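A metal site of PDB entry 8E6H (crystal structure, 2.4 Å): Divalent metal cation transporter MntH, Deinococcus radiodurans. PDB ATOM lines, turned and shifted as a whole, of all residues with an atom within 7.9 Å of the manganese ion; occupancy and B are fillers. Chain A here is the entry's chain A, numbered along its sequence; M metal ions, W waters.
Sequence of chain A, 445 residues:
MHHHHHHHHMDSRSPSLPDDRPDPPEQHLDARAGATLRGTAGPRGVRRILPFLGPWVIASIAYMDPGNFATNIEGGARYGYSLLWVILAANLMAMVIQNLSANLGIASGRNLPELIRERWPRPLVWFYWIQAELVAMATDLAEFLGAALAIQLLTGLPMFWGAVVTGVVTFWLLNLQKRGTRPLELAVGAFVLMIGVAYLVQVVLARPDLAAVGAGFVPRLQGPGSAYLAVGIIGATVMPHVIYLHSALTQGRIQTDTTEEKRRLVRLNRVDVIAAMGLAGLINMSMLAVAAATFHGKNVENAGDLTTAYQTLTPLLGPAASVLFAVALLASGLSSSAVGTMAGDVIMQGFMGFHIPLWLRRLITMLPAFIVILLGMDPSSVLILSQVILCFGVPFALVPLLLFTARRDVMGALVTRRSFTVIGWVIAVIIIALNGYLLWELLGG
N of Gly 67 sits close to OD2 of Asp 65, 3.4 Å away. The backbone carbonyl oxygen of Tyr 63 sits close to the side-chain amide oxygen of Asn 68, at 3.2 Å. The backbone carbonyl oxygen of Asn 68 is in hydrogen-bond range of the side-chain hydroxyl of Thr 71.
Tyr 63 touches the manganese ion. Of the 27 residues printed, 6 come within 4 Å of the manganese ion.
The manganese ion is bound by O of Ala 62, water W1, O of Ala 236, OD1 of Asn 68, OD1 of Asp 65 and SD of Met 239.
Water W1 lies within hydrogen-bond range of OE1 of Gln 387 (2.8 Å) and OD2 of Asp 65 (3.0 Å).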
ATOM      1  N   SER A  60     -32.988  -6.693  16.779  1.00  0.00           N
ATOM      2  CA  SER A  60     -33.283  -6.282  18.144  1.00  0.00           C
ATOM      3  C   SER A  60     -32.524  -7.084  19.183  1.00  0.00           C
ATOM      4  O   SER A  60     -32.616  -6.782  20.372  1.00  0.00           O
ATOM      5  CB  SER A  60     -34.788  -6.394  18.385  1.00  0.00           C
ATOM      6  OG  SER A  60     -35.485  -6.264  17.159  1.00  0.00           O
ATOM      7  N   ILE A  61     -31.752  -8.100  18.767  1.00  0.00           N
ATOM      8  CA  ILE A  61     -30.953  -8.889  19.695  1.00  0.00           C
ATOM      9  C   ILE A  61     -29.757  -8.114  20.240  1.00  0.00           C
ATOM     10  O   ILE A  61     -29.136  -8.562  21.209  1.00  0.00           O
ATOM     11  CB  ILE A  61     -30.495 -10.190  19.010  1.00  0.00           C
ATOM     12  CG1 ILE A  61     -30.073 -11.235  20.044  1.00  0.00           C
ATOM     13  CG2 ILE A  61     -29.386  -9.918  18.023  1.00  0.00           C
ATOM     14  CD1 ILE A  61     -31.215 -11.673  20.942  1.00  0.00           C
ATOM     15  N   ALA A  62     -29.423  -6.955  19.642  1.00  0.00           N
ATOM     16  CA  ALA A  62     -28.319  -6.143  20.145  1.00  0.00           C
ATOM     17  C   ALA A  62     -28.568  -5.662  21.566  1.00  0.00           C
ATOM     18  O   ALA A  62     -27.609  -5.479  22.341  1.00  0.00           O
ATOM     19  CB  ALA A  62     -28.074  -4.944  19.232  1.00  0.00           C
ATOM     20  N   TYR A  63     -29.825  -5.425  21.933  1.00  0.00           N
ATOM     21  CA  TYR A  63     -30.178  -5.059  23.301  1.00  0.00           C
ATOM     22  C   TYR A  63     -30.131  -6.246  24.247  1.00  0.00           C
ATOM     23  O   TYR A  63     -30.365  -6.071  25.450  1.00  0.00           O
ATOM     24  CB  TYR A  63     -31.566  -4.404  23.324  1.00  0.00           C
ATOM     25  CG  TYR A  63     -31.691  -3.247  22.361  1.00  0.00           C
ATOM     26  CD1 TYR A  63     -32.160  -3.435  21.061  1.00  0.00           C
ATOM     27  CD2 TYR A  63     -31.345  -1.959  22.743  1.00  0.00           C
ATOM     28  CE1 TYR A  63     -32.279  -2.379  20.181  1.00  0.00           C
ATOM     29  CE2 TYR A  63     -31.455  -0.898  21.861  1.00  0.00           C
ATOM     30  CZ  TYR A  63     -31.921  -1.110  20.585  1.00  0.00           C
ATOM     31  OH  TYR A  63     -32.031  -0.044  19.716  1.00  0.00           O
ATOM     32  N   MET A  64     -29.862  -7.446  23.741  1.00  0.00           N
ATOM     33  CA  MET A  64     -29.702  -8.651  24.547  1.00  0.00           C
ATOM     34  C   MET A  64     -28.497  -9.454  24.100  1.00  0.00           C
ATOM     35  O   MET A  64     -28.479 -10.685  24.232  1.00  0.00           O
ATOM     36  CB  MET A  64     -30.959  -9.513  24.513  1.00  0.00           C
ATOM     37  CG  MET A  64     -32.101  -8.997  25.369  1.00  0.00           C
ATOM     38  SD  MET A  64     -31.608  -8.823  27.097  1.00  0.00           S
ATOM     39  CE  MET A  64     -31.022 -10.478  27.465  1.00  0.00           C
ATOM     40  N   ASP A  65     -27.498  -8.777  23.531  1.00  0.00           N
ATOM     41  CA  ASP A  65     -26.284  -9.425  23.086  1.00  0.00           C
ATOM     42  C   ASP A  65     -25.448  -9.822  24.302  1.00  0.00           C
ATOM     43  O   ASP A  65     -25.735  -9.386  25.423  1.00  0.00           O
ATOM     44  CB  ASP A  65     -25.515  -8.497  22.132  1.00  0.00           C
ATOM     45  CG  ASP A  65     -24.747  -7.409  22.858  1.00  0.00           C
ATOM     46  OD1 ASP A  65     -25.289  -6.822  23.815  1.00  0.00           O
ATOM     47  OD2 ASP A  65     -23.597  -7.141  22.469  1.00  0.00           O
ATOM     48  N   PRO A  66     -24.420 -10.666  24.110  1.00  0.00           N
ATOM     49  CA  PRO A  66     -23.562 -11.047  25.245  1.00  0.00           C
ATOM     50  C   PRO A  66     -22.973  -9.864  26.007  1.00  0.00           C
ATOM     51  O   PRO A  66     -22.565 -10.024  27.168  1.00  0.00           O
ATOM     52  CB  PRO A  66     -22.466 -11.884  24.564  1.00  0.00           C
ATOM     53  CG  PRO A  66     -23.163 -12.497  23.408  1.00  0.00           C
ATOM     54  CD  PRO A  66     -24.131 -11.462  22.914  1.00  0.00           C
ATOM     55  N   GLY A  67     -22.914  -8.699  25.376  1.00  0.00           N
ATOM     56  CA  GLY A  67     -22.463  -7.508  26.079  1.00  0.00           C
ATOM     57  C   GLY A  67     -23.374  -7.110  27.223  1.00  0.00           C
ATOM     58  O   GLY A  67     -22.909  -6.673  28.270  1.00  0.00           O
ATOM     59  N   ASN A  68     -24.688  -7.263  27.035  1.00  0.00           N
ATOM     60  CA  ASN A  68     -25.628  -6.956  28.109  1.00  0.00           C
ATOM     61  C   ASN A  68     -25.547  -8.001  29.212  1.00  0.00           C
ATOM     62  O   ASN A  68     -25.633  -7.663  30.402  1.00  0.00           O
ATOM     63  CB  ASN A  68     -27.048  -6.851  27.562  1.00  0.00           C
ATOM     64  CG  ASN A  68     -27.251  -5.617  26.716  1.00  0.00           C
ATOM     65  OD1 ASN A  68     -27.227  -5.684  25.485  1.00  0.00           O
ATOM     66  ND2 ASN A  68     -27.456  -4.477  27.357  1.00  0.00           N
ATOM     67  N   PHE A  69     -25.383  -9.278  28.851  1.00  0.00           N
ATOM     68  CA  PHE A  69     -25.212 -10.321  29.853  1.00  0.00           C
ATOM     69  C   PHE A  69     -24.006 -10.043  30.744  1.00  0.00           C
ATOM     70  O   PHE A  69     -24.084 -10.156  31.969  1.00  0.00           O
ATOM     71  CB  PHE A  69     -25.068 -11.689  29.179  1.00  0.00           C
ATOM     72  CG  PHE A  69     -26.346 -12.221  28.589  1.00  0.00           C
ATOM     73  CD1 PHE A  69     -27.262 -12.890  29.381  1.00  0.00           C
ATOM     74  CD2 PHE A  69     -26.606 -12.076  27.241  1.00  0.00           C
ATOM     75  CE1 PHE A  69     -28.433 -13.390  28.844  1.00  0.00           C
ATOM     76  CE2 PHE A  69     -27.773 -12.568  26.694  1.00  0.00           C
ATOM     77  CZ  PHE A  69     -28.691 -13.230  27.490  1.00  0.00           C
ATOM     78  N   THR A  71     -22.361  -7.126  31.300  1.00  0.00           N
ATOM     79  CA  THR A  71     -22.457  -5.914  32.100  1.00  0.00           C
ATOM     80  C   THR A  71     -23.528  -6.008  33.177  1.00  0.00           C
ATOM     81  O   THR A  71     -23.367  -5.447  34.261  1.00  0.00           O
ATOM     82  CB  THR A  71     -22.725  -4.708  31.198  1.00  0.00           C
ATOM     83  OG1 THR A  71     -23.757  -5.027  30.249  1.00  0.00           O
ATOM     84  CG2 THR A  71     -21.464  -4.326  30.438  1.00  0.00           C
ATOM     85  N   THR A 139     -18.000  -4.054  18.645  1.00  0.00           N
ATOM     86  CA  THR A 139     -19.323  -4.658  18.749  1.00  0.00           C
ATOM     87  C   THR A 139     -19.271  -6.156  18.444  1.00  0.00           C
ATOM     88  O   THR A 139     -19.755  -6.976  19.220  1.00  0.00           O
ATOM     89  CB  THR A 139     -20.303  -3.969  17.804  1.00  0.00           C
ATOM     90  OG1 THR A 139     -20.305  -2.556  18.057  1.00  0.00           O
ATOM     91  CG2 THR A 139     -21.714  -4.504  18.013  1.00  0.00           C
ATOM     92  N   GLU A 143     -19.800 -10.027  20.805  1.00  0.00           N
ATOM     93  CA  GLU A 143     -20.812 -10.955  20.336  1.00  0.00           C
ATOM     94  C   GLU A 143     -20.193 -12.249  19.810  1.00  0.00           C
ATOM     95  O   GLU A 143     -20.696 -13.340  20.099  1.00  0.00           O
ATOM     96  CB  GLU A 143     -21.672 -10.290  19.268  1.00  0.00           C
ATOM     97  CG  GLU A 143     -22.301  -8.977  19.726  1.00  0.00           C
ATOM     98  CD  GLU A 143     -22.898  -8.185  18.588  1.00  0.00           C
ATOM     99  OE1 GLU A 143     -22.491  -8.406  17.428  1.00  0.00           O
ATOM    100  OE2 GLU A 143     -23.779  -7.340  18.852  1.00  0.00           O
ATOM    101  N   GLY A 232     -19.629   1.032  30.535  1.00  0.00           N
ATOM    102  CA  GLY A 232     -19.912  -0.183  29.784  1.00  0.00           C
ATOM    103  C   GLY A 232     -21.383  -0.494  29.683  1.00  0.00           C
ATOM    104  O   GLY A 232     -21.835  -1.043  28.678  1.00  0.00           O
ATOM    105  N   ILE A 233     -22.164  -0.160  30.720  1.00  0.00           N
ATOM    106  CA  ILE A 233     -23.598  -0.406  30.677  1.00  0.00           C
ATOM    107  C   ILE A 233     -24.264   0.516  29.650  1.00  0.00           C
ATOM    108  O   ILE A 233     -25.196   0.104  28.946  1.00  0.00           O
ATOM    109  CB  ILE A 233     -24.208  -0.242  32.083  1.00  0.00           C
ATOM    110  CG1 ILE A 233     -23.738  -1.373  32.997  1.00  0.00           C
ATOM    111  CG2 ILE A 233     -25.730  -0.199  32.016  1.00  0.00           C
ATOM    112  CD1 ILE A 233     -24.282  -1.283  34.406  1.00  0.00           C
ATOM    113  N   ILE A 234     -23.801   1.760  29.561  1.00  0.00           N
ATOM    114  CA  ILE A 234     -24.372   2.689  28.583  1.00  0.00           C
ATOM    115  C   ILE A 234     -24.057   2.233  27.159  1.00  0.00           C
ATOM    116  O   ILE A 234     -24.929   2.260  26.287  1.00  0.00           O
ATOM    117  CB  ILE A 234     -23.855   4.112  28.840  1.00  0.00           C
ATOM    118  CG1 ILE A 234     -24.271   4.583  30.239  1.00  0.00           C
ATOM    119  CG2 ILE A 234     -24.369   5.073  27.773  1.00  0.00           C
ATOM    120  CD1 ILE A 234     -23.922   6.019  30.519  1.00  0.00           C
ATOM    121  N   GLY A 235     -22.814   1.808  26.916  1.00  0.00           N
ATOM    122  CA  GLY A 235     -22.463   1.314  25.589  1.00  0.00           C
ATOM    123  C   GLY A 235     -23.182   0.026  25.232  1.00  0.00           C
ATOM    124  O   GLY A 235     -23.431  -0.231  24.051  1.00  0.00           O
ATOM    125  N   ALA A 236     -23.525  -0.791  26.230  1.00  0.00           N
ATOM    126  CA  ALA A 236     -24.235  -2.031  25.969  1.00  0.00           C
ATOM    127  C   ALA A 236     -25.692  -1.786  25.560  1.00  0.00           C
ATOM    128  O   ALA A 236     -26.290  -2.646  24.918  1.00  0.00           O
ATOM    129  CB  ALA A 236     -24.182  -2.937  27.195  1.00  0.00           C
ATOM    130  N   THR A 237     -26.254  -0.638  25.927  1.00  0.00           N
ATOM    131  CA  THR A 237     -27.616  -0.263  25.557  1.00  0.00           C
ATOM    132  C   THR A 237     -27.660   0.809  24.473  1.00  0.00           C
ATOM    133  O   THR A 237     -28.424   0.683  23.512  1.00  0.00           O
ATOM    134  CB  THR A 237     -28.386   0.232  26.789  1.00  0.00           C
ATOM    135  OG1 THR A 237     -28.439  -0.819  27.770  1.00  0.00           O
ATOM    136  CG2 THR A 237     -29.802   0.651  26.411  1.00  0.00           C
ATOM    137  N   VAL A 238     -26.858   1.869  24.618  1.00  0.00           N
ATOM    138  CA  VAL A 238     -26.747   2.887  23.580  1.00  0.00           C
ATOM    139  C   VAL A 238     -25.588   2.442  22.690  1.00  0.00           C
ATOM    140  O   VAL A 238     -24.432   2.754  22.942  1.00  0.00           O
ATOM    141  CB  VAL A 238     -26.544   4.282  24.159  1.00  0.00           C
ATOM    142  CG1 VAL A 238     -26.552   5.311  23.045  1.00  0.00           C
ATOM    143  CG2 VAL A 238     -27.639   4.589  25.176  1.00  0.00           C
ATOM    144  N   MET A 239     -25.923   1.710  21.637  1.00  0.00           N
ATOM    145  CA  MET A 239     -24.926   1.109  20.756  1.00  0.00           C
ATOM    146  C   MET A 239     -24.784   1.936  19.495  1.00  0.00           C
ATOM    147  O   MET A 239     -25.780   2.171  18.797  1.00  0.00           O
ATOM    148  CB  MET A 239     -25.319  -0.332  20.411  1.00  0.00           C
ATOM    149  CG  MET A 239     -25.736  -1.154  21.640  1.00  0.00           C
ATOM    150  SD  MET A 239     -25.823  -2.924  21.313  1.00  0.00           S
ATOM    151  CE  MET A 239     -24.091  -3.337  21.211  1.00  0.00           C
ATOM    152  N   HIS A 241     -23.536   1.304  16.517  1.00  0.00           N
ATOM    153  CA  HIS A 241     -23.859   0.632  15.267  1.00  0.00           C
ATOM    154  C   HIS A 241     -25.364   0.585  15.022  1.00  0.00           C
ATOM    155  O   HIS A 241     -25.809   0.578  13.865  1.00  0.00           O
ATOM    156  CB  HIS A 241     -23.268  -0.774  15.254  1.00  0.00           C
ATOM    157  CG  HIS A 241     -24.059  -1.775  16.038  1.00  0.00           C
ATOM    158  ND1 HIS A 241     -23.934  -1.906  17.408  1.00  0.00           N
ATOM    159  CD2 HIS A 241     -24.973  -2.689  15.652  1.00  0.00           C
ATOM    160  CE1 HIS A 241     -24.738  -2.863  17.828  1.00  0.00           C
ATOM    161  NE2 HIS A 241     -25.390  -3.354  16.784  1.00  0.00           N
ATOM    162  N   VAL A 242     -26.167   0.561  16.096  1.00  0.00           N
ATOM    163  CA  VAL A 242     -27.611   0.586  15.936  1.00  0.00           C
ATOM    164  C   VAL A 242     -28.076   1.986  15.548  1.00  0.00           C
ATOM    165  O   VAL A 242     -29.085   2.142  14.835  1.00  0.00           O
ATOM    166  CB  VAL A 242     -28.314   0.106  17.224  1.00  0.00           C
ATOM    167  CG1 VAL A 242     -29.815   0.076  17.041  1.00  0.00           C
ATOM    168  CG2 VAL A 242     -27.794  -1.264  17.615  1.00  0.00           C
ATOM    169  N   ASN A 284     -33.020  -6.224  31.506  1.00  0.00           N
ATOM    170  CA  ASN A 284     -31.652  -5.872  31.911  1.00  0.00           C
ATOM    171  C   ASN A 284     -31.595  -5.505  33.389  1.00  0.00           C
ATOM    172  O   ASN A 284     -30.658  -5.928  34.091  1.00  0.00           O
ATOM    173  CB  ASN A 284     -31.135  -4.713  31.052  1.00  0.00           C
ATOM    174  CG  ASN A 284     -30.759  -5.147  29.648  1.00  0.00           C
ATOM    175  OD1 ASN A 284     -30.301  -6.269  29.432  1.00  0.00           O
ATOM    176  ND2 ASN A 284     -30.947  -4.248  28.686  1.00  0.00           N
ATOM    177  N   SER A 336     -26.512 -11.817  16.842  1.00  0.00           N
ATOM    178  CA  SER A 336     -26.004 -10.445  16.878  1.00  0.00           C
ATOM    179  C   SER A 336     -24.736 -10.309  16.052  1.00  0.00           C
ATOM    180  O   SER A 336     -24.523  -9.267  15.418  1.00  0.00           O
ATOM    181  CB  SER A 336     -25.755 -10.022  18.329  1.00  0.00           C
ATOM    182  OG  SER A 336     -24.831 -10.896  18.960  1.00  0.00           O
ATOM    183  N   GLN A 387     -17.797  -3.003  25.402  1.00  0.00           N
ATOM    184  CA  GLN A 387     -18.926  -2.111  25.640  1.00  0.00           C
ATOM    185  C   GLN A 387     -18.446  -0.739  26.107  1.00  0.00           C
ATOM    186  O   GLN A 387     -19.048   0.286  25.758  1.00  0.00           O
ATOM    187  CB  GLN A 387     -19.875  -2.728  26.669  1.00  0.00           C
ATOM    188  CG  GLN A 387     -20.321  -4.139  26.344  1.00  0.00           C
ATOM    189  CD  GLN A 387     -20.860  -4.270  24.934  1.00  0.00           C
ATOM    190  OE1 GLN A 387     -21.711  -3.492  24.511  1.00  0.00           O
ATOM    191  NE2 GLN A 387     -20.359  -5.243  24.192  1.00  0.00           N
ATOM    192  N   LEU A 390     -17.355   1.006  23.082  1.00  0.00           N
ATOM    193  CA  LEU A 390     -18.509   1.397  22.277  1.00  0.00           C
ATOM    194  C   LEU A 390     -19.095   2.725  22.759  1.00  0.00           C
ATOM    195  O   LEU A 390     -19.569   3.531  21.945  1.00  0.00           O
ATOM    196  CB  LEU A 390     -19.570   0.303  22.318  1.00  0.00           C
ATOM    197  CG  LEU A 390     -19.287  -0.933  21.461  1.00  0.00           C
ATOM    198  CD1 LEU A 390     -20.504  -1.856  21.434  1.00  0.00           C
ATOM    199  CD2 LEU A 390     -18.873  -0.528  20.057  1.00  0.00           C
HETATM  200 MN    MN M   1     -26.265  -4.431  23.588  1.00  0.00          MN
HETATM  201  O   HOH W   1     -24.163  -4.757  24.215  1.00  0.00           O
